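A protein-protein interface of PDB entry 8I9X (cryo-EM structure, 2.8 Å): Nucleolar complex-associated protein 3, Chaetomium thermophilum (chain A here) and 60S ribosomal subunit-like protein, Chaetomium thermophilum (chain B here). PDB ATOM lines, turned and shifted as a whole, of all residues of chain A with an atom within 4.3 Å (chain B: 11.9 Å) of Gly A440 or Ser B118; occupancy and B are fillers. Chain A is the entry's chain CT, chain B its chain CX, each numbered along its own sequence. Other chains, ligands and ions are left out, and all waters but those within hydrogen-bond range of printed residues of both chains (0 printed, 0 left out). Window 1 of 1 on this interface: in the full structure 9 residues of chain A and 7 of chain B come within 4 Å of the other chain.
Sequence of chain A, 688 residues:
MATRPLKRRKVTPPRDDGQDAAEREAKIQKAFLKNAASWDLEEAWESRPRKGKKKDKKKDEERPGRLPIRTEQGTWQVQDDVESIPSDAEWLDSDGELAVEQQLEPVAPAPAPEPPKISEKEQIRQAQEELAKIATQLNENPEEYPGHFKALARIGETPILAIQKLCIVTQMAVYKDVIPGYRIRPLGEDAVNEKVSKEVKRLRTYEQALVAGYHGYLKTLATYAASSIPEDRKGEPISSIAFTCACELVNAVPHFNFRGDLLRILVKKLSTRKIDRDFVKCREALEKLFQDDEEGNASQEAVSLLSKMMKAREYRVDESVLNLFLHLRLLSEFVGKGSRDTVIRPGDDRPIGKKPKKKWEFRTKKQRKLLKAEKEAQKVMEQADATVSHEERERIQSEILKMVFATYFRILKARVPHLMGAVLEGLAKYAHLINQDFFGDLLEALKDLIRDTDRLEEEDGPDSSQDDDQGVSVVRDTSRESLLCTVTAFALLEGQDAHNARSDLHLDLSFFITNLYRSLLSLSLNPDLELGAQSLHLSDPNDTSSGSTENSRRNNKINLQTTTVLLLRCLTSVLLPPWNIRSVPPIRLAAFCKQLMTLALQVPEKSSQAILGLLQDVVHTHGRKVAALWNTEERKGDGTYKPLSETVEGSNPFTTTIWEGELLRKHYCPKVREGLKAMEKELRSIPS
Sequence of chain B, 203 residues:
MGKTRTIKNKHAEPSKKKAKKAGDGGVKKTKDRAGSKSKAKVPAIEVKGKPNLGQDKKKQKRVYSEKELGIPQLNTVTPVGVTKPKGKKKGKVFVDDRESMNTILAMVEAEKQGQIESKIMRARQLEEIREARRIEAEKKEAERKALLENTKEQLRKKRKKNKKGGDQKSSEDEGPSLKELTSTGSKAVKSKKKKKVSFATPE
Asp A437 touches Glu B117 (CB to O, 3.6 Å).
CA of Gly A440 touches OG of Ser B118 (3.3 Å).
Asp A441 touches Ser B118.
CG of Met B121 touches OE2 of Glu A444 (3.1 Å).
The backbone carbonyl oxygen (O) of Gly A440 sits close to the side-chain carboxylate (OE1) of Glu A444.
OG of Ser B118 sits close to SD of Met B121 (3.7 Å).
Of chain A, only Asp A437 (3.0 Å), Gly A440 (3.3 Å) and Asp A441 (3.7 Å) come within 4 Å of Ser B118.
Asp A437 touches two residues of chain B.
No residue of chain B comes within 4 Å of Phe A439.
Of chain B, only Ser B118 and Ile B120 come within 4 Å of Asp A441.
No residue of chain B comes within 4 Å of Leu A442.
No residue of chain B comes within 4 Å of Leu A443.
Glu A444 touches just one residue of chain B: Met B121.
Of the printed residues of chain A, Glu B117 touches Gln A436 and Asp A437.
Of the printed residues of chain A, Ile B120 touches Asp A441 (3.2 Å).
Of the printed residues of chain B, Gln A436 touches Glu B117.
Of the printed residues of chain A, Met B121 touches Glu A444 (3.1 Å).
Glu B127 touches none of the printed residues of chain A.
Gln B125 touches none of the printed residues of chain A.
The nearest printed residue of chain A that does not touch Glu B117 is Phe A438 (6.3 Å).
The side-chain carboxylate (OE1) of Glu B117 sits close to the side-chain amide oxygen (OE1) of Gln A436, 3.5 Å away.
The side-chain hydroxyl of Ser B118 is in hydrogen-bond range of the backbone carbonyl oxygen of Asp A437, at 3.0 Å.
The backbone NH of Ile B120 sits close to the side-chain carboxylate of Asp A441 (3.5 Å).
Printed residues of chain A that touch a printed residue of chain B: Gln A436, Asp A437, Gly A440, Asp A441 and Glu A444.
Along chain A the printed residues that touch a printed residue of chain B span positions 436 to 444.
Of the 17 printed residues of chain B, 4 touch a printed residue of chain A.
Printed residues of chain B that touch a printed residue of chain A: Glu B117, Ser B118, Ile B120 and Met B121.
Among the printed residues, 7 pairs touch across the chains.
Among the printed residues, no Asp or Glu carboxylate lies within 4 Å of a Lys or Arg side-chain nitrogen of the other chain.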
ATOM      1  N   GLN A 436     -18.547 -24.507  13.133  1.00  0.00           N
ATOM      2  CA  GLN A 436     -19.840 -25.183  13.095  1.00  0.00           C
ATOM      3  C   GLN A 436     -20.511 -25.026  11.730  1.00  0.00           C
ATOM      4  O   GLN A 436     -20.889 -26.016  11.075  1.00  0.00           O
ATOM      5  CB  GLN A 436     -20.703 -24.602  14.213  1.00  0.00           C
ATOM      6  CG  GLN A 436     -21.683 -25.543  14.850  1.00  0.00           C
ATOM      7  CD  GLN A 436     -22.293 -24.956  16.107  1.00  0.00           C
ATOM      8  OE1 GLN A 436     -22.038 -23.804  16.452  1.00  0.00           O
ATOM      9  NE2 GLN A 436     -23.104 -25.749  16.798  1.00  0.00           N
ATOM     10  N   ASP A 437     -20.674 -23.778  11.284  1.00  0.00           N
ATOM     11  CA  ASP A 437     -21.156 -23.539   9.931  1.00  0.00           C
ATOM     12  C   ASP A 437     -20.290 -24.248   8.906  1.00  0.00           C
ATOM     13  O   ASP A 437     -20.802 -24.709   7.880  1.00  0.00           O
ATOM     14  CB  ASP A 437     -21.200 -22.038   9.641  1.00  0.00           C
ATOM     15  CG  ASP A 437     -19.876 -21.352   9.913  1.00  0.00           C
ATOM     16  OD1 ASP A 437     -18.955 -22.015  10.433  1.00  0.00           O
ATOM     17  OD2 ASP A 437     -19.755 -20.148   9.604  1.00  0.00           O
ATOM     18  N   PHE A 438     -18.997 -24.378   9.177  1.00  0.00           N
ATOM     19  CA  PHE A 438     -18.117 -25.205   8.373  1.00  0.00           C
ATOM     20  C   PHE A 438     -18.488 -26.679   8.431  1.00  0.00           C
ATOM     21  O   PHE A 438     -18.308 -27.382   7.438  1.00  0.00           O
ATOM     22  CB  PHE A 438     -16.664 -25.008   8.812  1.00  0.00           C
ATOM     23  CG  PHE A 438     -16.169 -23.601   8.640  1.00  0.00           C
ATOM     24  CD1 PHE A 438     -16.793 -22.738   7.755  1.00  0.00           C
ATOM     25  CD2 PHE A 438     -15.090 -23.139   9.366  1.00  0.00           C
ATOM     26  CE1 PHE A 438     -16.346 -21.444   7.596  1.00  0.00           C
ATOM     27  CE2 PHE A 438     -14.639 -21.843   9.210  1.00  0.00           C
ATOM     28  CZ  PHE A 438     -15.268 -20.997   8.324  1.00  0.00           C
ATOM     29  N   PHE A 439     -19.007 -27.168   9.560  1.00  0.00           N
ATOM     30  CA  PHE A 439     -19.492 -28.544   9.596  1.00  0.00           C
ATOM     31  C   PHE A 439     -20.648 -28.734   8.624  1.00  0.00           C
ATOM     32  O   PHE A 439     -20.668 -29.699   7.840  1.00  0.00           O
ATOM     33  CB  PHE A 439     -19.914 -28.914  11.018  1.00  0.00           C
ATOM     34  CG  PHE A 439     -19.870 -30.382  11.305  1.00  0.00           C
ATOM     35  CD1 PHE A 439     -20.924 -31.204  10.949  1.00  0.00           C
ATOM     36  CD2 PHE A 439     -18.776 -30.942  11.938  1.00  0.00           C
ATOM     37  CE1 PHE A 439     -20.885 -32.557  11.217  1.00  0.00           C
ATOM     38  CE2 PHE A 439     -18.731 -32.292  12.209  1.00  0.00           C
ATOM     39  CZ  PHE A 439     -19.786 -33.102  11.848  1.00  0.00           C
ATOM     40  N   GLY A 440     -21.600 -27.800   8.633  1.00  0.00           N
ATOM     41  CA  GLY A 440     -22.617 -27.837   7.592  1.00  0.00           C
ATOM     42  C   GLY A 440     -22.054 -27.759   6.183  1.00  0.00           C
ATOM     43  O   GLY A 440     -22.494 -28.509   5.298  1.00  0.00           O
ATOM     44  N   ASP A 441     -21.078 -26.876   5.966  1.00  0.00           N
ATOM     45  CA  ASP A 441     -20.462 -26.739   4.654  1.00  0.00           C
ATOM     46  C   ASP A 441     -19.814 -28.032   4.180  1.00  0.00           C
ATOM     47  O   ASP A 441     -19.943 -28.373   3.006  1.00  0.00           O
ATOM     48  CB  ASP A 441     -19.428 -25.614   4.670  1.00  0.00           C
ATOM     49  CG  ASP A 441     -20.027 -24.277   5.064  1.00  0.00           C
ATOM     50  OD1 ASP A 441     -21.257 -24.110   4.922  1.00  0.00           O
ATOM     51  OD2 ASP A 441     -19.269 -23.394   5.515  1.00  0.00           O
ATOM     52  N   LEU A 442     -19.115 -28.753   5.059  1.00  0.00           N
ATOM     53  CA  LEU A 442     -18.629 -30.085   4.715  1.00  0.00           C
ATOM     54  C   LEU A 442     -19.750 -31.069   4.415  1.00  0.00           C
ATOM     55  O   LEU A 442     -19.574 -31.933   3.548  1.00  0.00           O
ATOM     56  CB  LEU A 442     -17.734 -30.656   5.821  1.00  0.00           C
ATOM     57  CG  LEU A 442     -16.249 -30.264   5.883  1.00  0.00           C
ATOM     58  CD1 LEU A 442     -15.988 -28.836   6.306  1.00  0.00           C
ATOM     59  CD2 LEU A 442     -15.508 -31.226   6.802  1.00  0.00           C
ATOM     60  N   LEU A 443     -20.892 -30.971   5.101  1.00  0.00           N
ATOM     61  CA  LEU A 443     -21.994 -31.859   4.726  1.00  0.00           C
ATOM     62  C   LEU A 443     -22.438 -31.638   3.281  1.00  0.00           C
ATOM     63  O   LEU A 443     -22.536 -32.598   2.503  1.00  0.00           O
ATOM     64  CB  LEU A 443     -23.176 -31.689   5.678  1.00  0.00           C
ATOM     65  CG  LEU A 443     -23.161 -32.632   6.880  1.00  0.00           C
ATOM     66  CD1 LEU A 443     -24.493 -32.595   7.602  1.00  0.00           C
ATOM     67  CD2 LEU A 443     -22.829 -34.046   6.439  1.00  0.00           C
ATOM     68  N   GLU A 444     -22.689 -30.388   2.886  1.00  0.00           N
ATOM     69  CA  GLU A 444     -23.046 -30.182   1.477  1.00  0.00           C
ATOM     70  C   GLU A 444     -21.863 -30.350   0.523  1.00  0.00           C
ATOM     71  O   GLU A 444     -22.073 -30.607  -0.667  1.00  0.00           O
ATOM     72  CB  GLU A 444     -23.758 -28.846   1.242  1.00  0.00           C
ATOM     73  CG  GLU A 444     -25.231 -28.841   1.671  1.00  0.00           C
ATOM     74  CD  GLU A 444     -25.475 -28.601   3.130  1.00  0.00           C
ATOM     75  OE1 GLU A 444     -24.511 -28.348   3.862  1.00  0.00           O
ATOM     76  OE2 GLU A 444     -26.647 -28.692   3.551  1.00  0.00           O
ATOM     77  N   ALA B 110     -38.957 -22.819   2.838  1.00  0.00           N
ATOM     78  CA  ALA B 110     -37.939 -21.834   3.186  1.00  0.00           C
ATOM     79  C   ALA B 110     -38.337 -21.043   4.424  1.00  0.00           C
ATOM     80  O   ALA B 110     -37.584 -20.986   5.407  1.00  0.00           O
ATOM     81  CB  ALA B 110     -37.689 -20.895   2.006  1.00  0.00           C
ATOM     82  N   GLN B 113     -38.340 -23.545   7.585  1.00  0.00           N
ATOM     83  CA  GLN B 113     -37.041 -23.873   8.164  1.00  0.00           C
ATOM     84  C   GLN B 113     -36.394 -22.642   8.786  1.00  0.00           C
ATOM     85  O   GLN B 113     -35.931 -22.680   9.931  1.00  0.00           O
ATOM     86  CB  GLN B 113     -36.136 -24.495   7.099  1.00  0.00           C
ATOM     87  CG  GLN B 113     -34.786 -24.960   7.617  1.00  0.00           C
ATOM     88  CD  GLN B 113     -33.947 -25.623   6.543  1.00  0.00           C
ATOM     89  OE1 GLN B 113     -34.355 -25.710   5.386  1.00  0.00           O
ATOM     90  NE2 GLN B 113     -32.770 -26.106   6.925  1.00  0.00           N
ATOM     91  N   GLY B 114     -36.357 -21.537   8.049  1.00  0.00           N
ATOM     92  CA  GLY B 114     -35.933 -20.267   8.622  1.00  0.00           C
ATOM     93  C   GLY B 114     -34.422 -20.139   8.721  1.00  0.00           C
ATOM     94  O   GLY B 114     -33.721 -20.192   7.709  1.00  0.00           O
ATOM     95  N   GLN B 115     -33.924 -19.969   9.946  1.00  0.00           N
ATOM     96  CA  GLN B 115     -32.556 -19.510  10.182  1.00  0.00           C
ATOM     97  C   GLN B 115     -31.586 -20.683  10.119  1.00  0.00           C
ATOM     98  O   GLN B 115     -31.785 -21.705  10.786  1.00  0.00           O
ATOM     99  CB  GLN B 115     -32.455 -18.805  11.530  1.00  0.00           C
ATOM    100  CG  GLN B 115     -31.182 -17.988  11.703  1.00  0.00           C
ATOM    101  CD  GLN B 115     -30.901 -17.086  10.515  1.00  0.00           C
ATOM    102  OE1 GLN B 115     -31.680 -16.185  10.209  1.00  0.00           O
ATOM    103  NE2 GLN B 115     -29.782 -17.326   9.839  1.00  0.00           N
ATOM    104  N   ILE B 116     -30.534 -20.534   9.321  1.00  0.00           N
ATOM    105  CA  ILE B 116     -29.508 -21.559   9.174  1.00  0.00           C
ATOM    106  C   ILE B 116     -28.144 -20.926   9.414  1.00  0.00           C
ATOM    107  O   ILE B 116     -27.838 -19.860   8.866  1.00  0.00           O
ATOM    108  CB  ILE B 116     -29.575 -22.206   7.781  1.00  0.00           C
ATOM    109  CG1 ILE B 116     -30.916 -22.915   7.575  1.00  0.00           C
ATOM    110  CG2 ILE B 116     -28.442 -23.194   7.617  1.00  0.00           C
ATOM    111  CD1 ILE B 116     -31.162 -23.351   6.141  1.00  0.00           C
ATOM    112  N   GLU B 117     -27.320 -21.581  10.235  1.00  0.00           N
ATOM    113  CA  GLU B 117     -25.982 -21.064  10.505  1.00  0.00           C
ATOM    114  C   GLU B 117     -25.078 -21.182   9.283  1.00  0.00           C
ATOM    115  O   GLU B 117     -24.243 -20.303   9.036  1.00  0.00           O
ATOM    116  CB  GLU B 117     -25.370 -21.794  11.700  1.00  0.00           C
ATOM    117  CG  GLU B 117     -24.002 -21.274  12.113  1.00  0.00           C
ATOM    118  CD  GLU B 117     -23.447 -21.985  13.334  1.00  0.00           C
ATOM    119  OE1 GLU B 117     -24.119 -22.900  13.851  1.00  0.00           O
ATOM    120  OE2 GLU B 117     -22.334 -21.627  13.778  1.00  0.00           O
ATOM    121  N   SER B 118     -25.226 -22.252   8.505  1.00  0.00           N
ATOM    122  CA  SER B 118     -24.298 -22.502   7.410  1.00  0.00           C
ATOM    123  C   SER B 118     -24.648 -21.674   6.177  1.00  0.00           C
ATOM    124  O   SER B 118     -25.759 -21.744   5.632  1.00  0.00           O
ATOM    125  CB  SER B 118     -24.281 -23.986   7.057  1.00  0.00           C
ATOM    126  OG  SER B 118     -23.817 -24.761   8.147  1.00  0.00           O
ATOM    127  N   LYS B 119     -23.659 -20.905   5.724  1.00  0.00           N
ATOM    128  CA  LYS B 119     -23.788 -20.083   4.531  1.00  0.00           C
ATOM    129  C   LYS B 119     -24.080 -20.904   3.287  1.00  0.00           C
ATOM    130  O   LYS B 119     -24.925 -20.509   2.474  1.00  0.00           O
ATOM    131  CB  LYS B 119     -22.506 -19.275   4.313  1.00  0.00           C
ATOM    132  CG  LYS B 119     -22.362 -18.075   5.225  1.00  0.00           C
ATOM    133  CD  LYS B 119     -21.100 -17.291   4.902  1.00  0.00           C
ATOM    134  CE  LYS B 119     -20.359 -16.888   6.166  1.00  0.00           C
ATOM    135  NZ  LYS B 119     -21.247 -16.162   7.117  1.00  0.00           N
ATOM    136  N   ILE B 120     -23.399 -22.040   3.120  1.00  0.00           N
ATOM    137  CA  ILE B 120     -23.651 -22.884   1.959  1.00  0.00           C
ATOM    138  C   ILE B 120     -25.062 -23.455   2.005  1.00  0.00           C
ATOM    139  O   ILE B 120     -25.727 -23.563   0.972  1.00  0.00           O
ATOM    140  CB  ILE B 120     -22.587 -23.991   1.856  1.00  0.00           C
ATOM    141  CG1 ILE B 120     -21.187 -23.373   1.820  1.00  0.00           C
ATOM    142  CG2 ILE B 120     -22.825 -24.853   0.627  1.00  0.00           C
ATOM    143  CD1 ILE B 120     -20.109 -24.326   1.353  1.00  0.00           C
ATOM    144  N   MET B 121     -25.546 -23.826   3.193  1.00  0.00           N
ATOM    145  CA  MET B 121     -26.915 -24.323   3.298  1.00  0.00           C
ATOM    146  C   MET B 121     -27.926 -23.253   2.908  1.00  0.00           C
ATOM    147  O   MET B 121     -28.893 -23.532   2.182  1.00  0.00           O
ATOM    148  CB  MET B 121     -27.197 -24.820   4.716  1.00  0.00           C
ATOM    149  CG  MET B 121     -26.411 -26.046   5.118  1.00  0.00           C
ATOM    150  SD  MET B 121     -26.722 -26.538   6.819  1.00  0.00           S
ATOM    151  CE  MET B 121     -28.400 -27.143   6.675  1.00  0.00           C
ATOM    152  N   ARG B 122     -27.724 -22.019   3.381  1.00  0.00           N
ATOM    153  CA  ARG B 122     -28.612 -20.932   2.977  1.00  0.00           C
ATOM    154  C   ARG B 122     -28.562 -20.715   1.468  1.00  0.00           C
ATOM    155  O   ARG B 122     -29.603 -20.519   0.819  1.00  0.00           O
ATOM    156  CB  ARG B 122     -28.238 -19.652   3.721  1.00  0.00           C
ATOM    157  CG  ARG B 122     -28.387 -19.758   5.228  1.00  0.00           C
ATOM    158  CD  ARG B 122     -28.316 -18.398   5.899  1.00  0.00           C
ATOM    159  NE  ARG B 122     -27.033 -17.744   5.673  1.00  0.00           N
ATOM    160  CZ  ARG B 122     -26.279 -17.228   6.633  1.00  0.00           C
ATOM    161  NH1 ARG B 122     -26.641 -17.286   7.904  1.00  0.00           N
ATOM    162  NH2 ARG B 122     -25.130 -16.643   6.311  1.00  0.00           N
ATOM    163  N   ALA B 123     -27.358 -20.761   0.894  1.00  0.00           N
ATOM    164  CA  ALA B 123     -27.212 -20.597  -0.547  1.00  0.00           C
ATOM    165  C   ALA B 123     -27.943 -21.694  -1.307  1.00  0.00           C
ATOM    166  O   ALA B 123     -28.582 -21.424  -2.325  1.00  0.00           O
ATOM    167  CB  ALA B 123     -25.732 -20.576  -0.924  1.00  0.00           C
ATOM    168  N   ARG B 124     -27.861 -22.939  -0.832  1.00  0.00           N
ATOM    169  CA  ARG B 124     -28.549 -24.036  -1.508  1.00  0.00           C
ATOM    170  C   ARG B 124     -30.061 -23.903  -1.408  1.00  0.00           C
ATOM    171  O   ARG B 124     -30.773 -24.242  -2.359  1.00  0.00           O
ATOM    172  CB  ARG B 124     -28.107 -25.386  -0.947  1.00  0.00           C
ATOM    173  CG  ARG B 124     -26.618 -25.611  -0.986  1.00  0.00           C
ATOM    174  CD  ARG B 124     -26.220 -26.530  -2.111  1.00  0.00           C
ATOM    175  NE  ARG B 124     -24.844 -26.287  -2.523  1.00  0.00           N
ATOM    176  CZ  ARG B 124     -24.106 -27.149  -3.207  1.00  0.00           C
ATOM    177  NH1 ARG B 124     -24.581 -28.328  -3.571  1.00  0.00           N
ATOM    178  NH2 ARG B 124     -22.861 -26.818  -3.535  1.00  0.00           N
ATOM    179  N   GLN B 125     -30.570 -23.431  -0.270  1.00  0.00           N
ATOM    180  CA  GLN B 125     -32.006 -23.189  -0.159  1.00  0.00           C
ATOM    181  C   GLN B 125     -32.458 -22.145  -1.178  1.00  0.00           C
ATOM    182  O   GLN B 125     -33.437 -22.346  -1.921  1.00  0.00           O
ATOM    183  CB  GLN B 125     -32.333 -22.744   1.267  1.00  0.00           C
ATOM    184  CG  GLN B 125     -33.801 -22.755   1.623  1.00  0.00           C
ATOM    185  CD  GLN B 125     -34.020 -22.816   3.120  1.00  0.00           C
ATOM    186  OE1 GLN B 125     -33.731 -21.861   3.840  1.00  0.00           O
ATOM    187  NE2 GLN B 125     -34.528 -23.944   3.599  1.00  0.00           N
ATOM    188  N   LEU B 126     -31.725 -21.034  -1.253  1.00  0.00           N
ATOM    189  CA  LEU B 126     -32.066 -20.013  -2.235  1.00  0.00           C
ATOM    190  C   LEU B 126     -31.939 -20.546  -3.657  1.00  0.00           C
ATOM    191  O   LEU B 126     -32.780 -20.240  -4.508  1.00  0.00           O
ATOM    192  CB  LEU B 126     -31.193 -18.776  -2.036  1.00  0.00           C
ATOM    193  CG  LEU B 126     -31.557 -17.938  -0.809  1.00  0.00           C
ATOM    194  CD1 LEU B 126     -30.428 -16.988  -0.443  1.00  0.00           C
ATOM    195  CD2 LEU B 126     -32.859 -17.185  -1.021  1.00  0.00           C
ATOM    196  N   GLU B 127     -30.915 -21.357  -3.927  1.00  0.00           N
ATOM    197  CA  GLU B 127     -30.721 -21.928  -5.254  1.00  0.00           C
ATOM    198  C   GLU B 127     -31.837 -22.882  -5.649  1.00  0.00           C
ATOM    199  O   GLU B 127     -32.224 -22.907  -6.819  1.00  0.00           O
ATOM    200  CB  GLU B 127     -29.375 -22.649  -5.336  1.00  0.00           C
ATOM    201  CG  GLU B 127     -28.169 -21.727  -5.372  1.00  0.00           C
ATOM    202  CD  GLU B 127     -28.072 -20.945  -6.668  1.00  0.00           C
ATOM    203  OE1 GLU B 127     -28.497 -21.473  -7.715  1.00  0.00           O
ATOM    204  OE2 GLU B 127     -27.569 -19.802  -6.637  1.00  0.00           O
ATOM    205  N   GLU B 128     -32.348 -23.690  -4.718  1.00  0.00           N
ATOM    206  CA  GLU B 128     -33.453 -24.564  -5.096  1.00  0.00           C
ATOM    207  C   GLU B 128     -34.718 -23.764  -5.369  1.00  0.00           C
ATOM    208  O   GLU B 128     -35.463 -24.096  -6.301  1.00  0.00           O
ATOM    209  CB  GLU B 128     -33.706 -25.638  -4.032  1.00  0.00           C
ATOM    210  CG  GLU B 128     -34.198 -25.144  -2.692  1.00  0.00           C
ATOM    211  CD  GLU B 128     -34.361 -26.264  -1.685  1.00  0.00           C
ATOM    212  OE1 GLU B 128     -34.064 -27.425  -2.034  1.00  0.00           O
ATOM    213  OE2 GLU B 128     -34.785 -25.983  -0.544  1.00  0.00           O
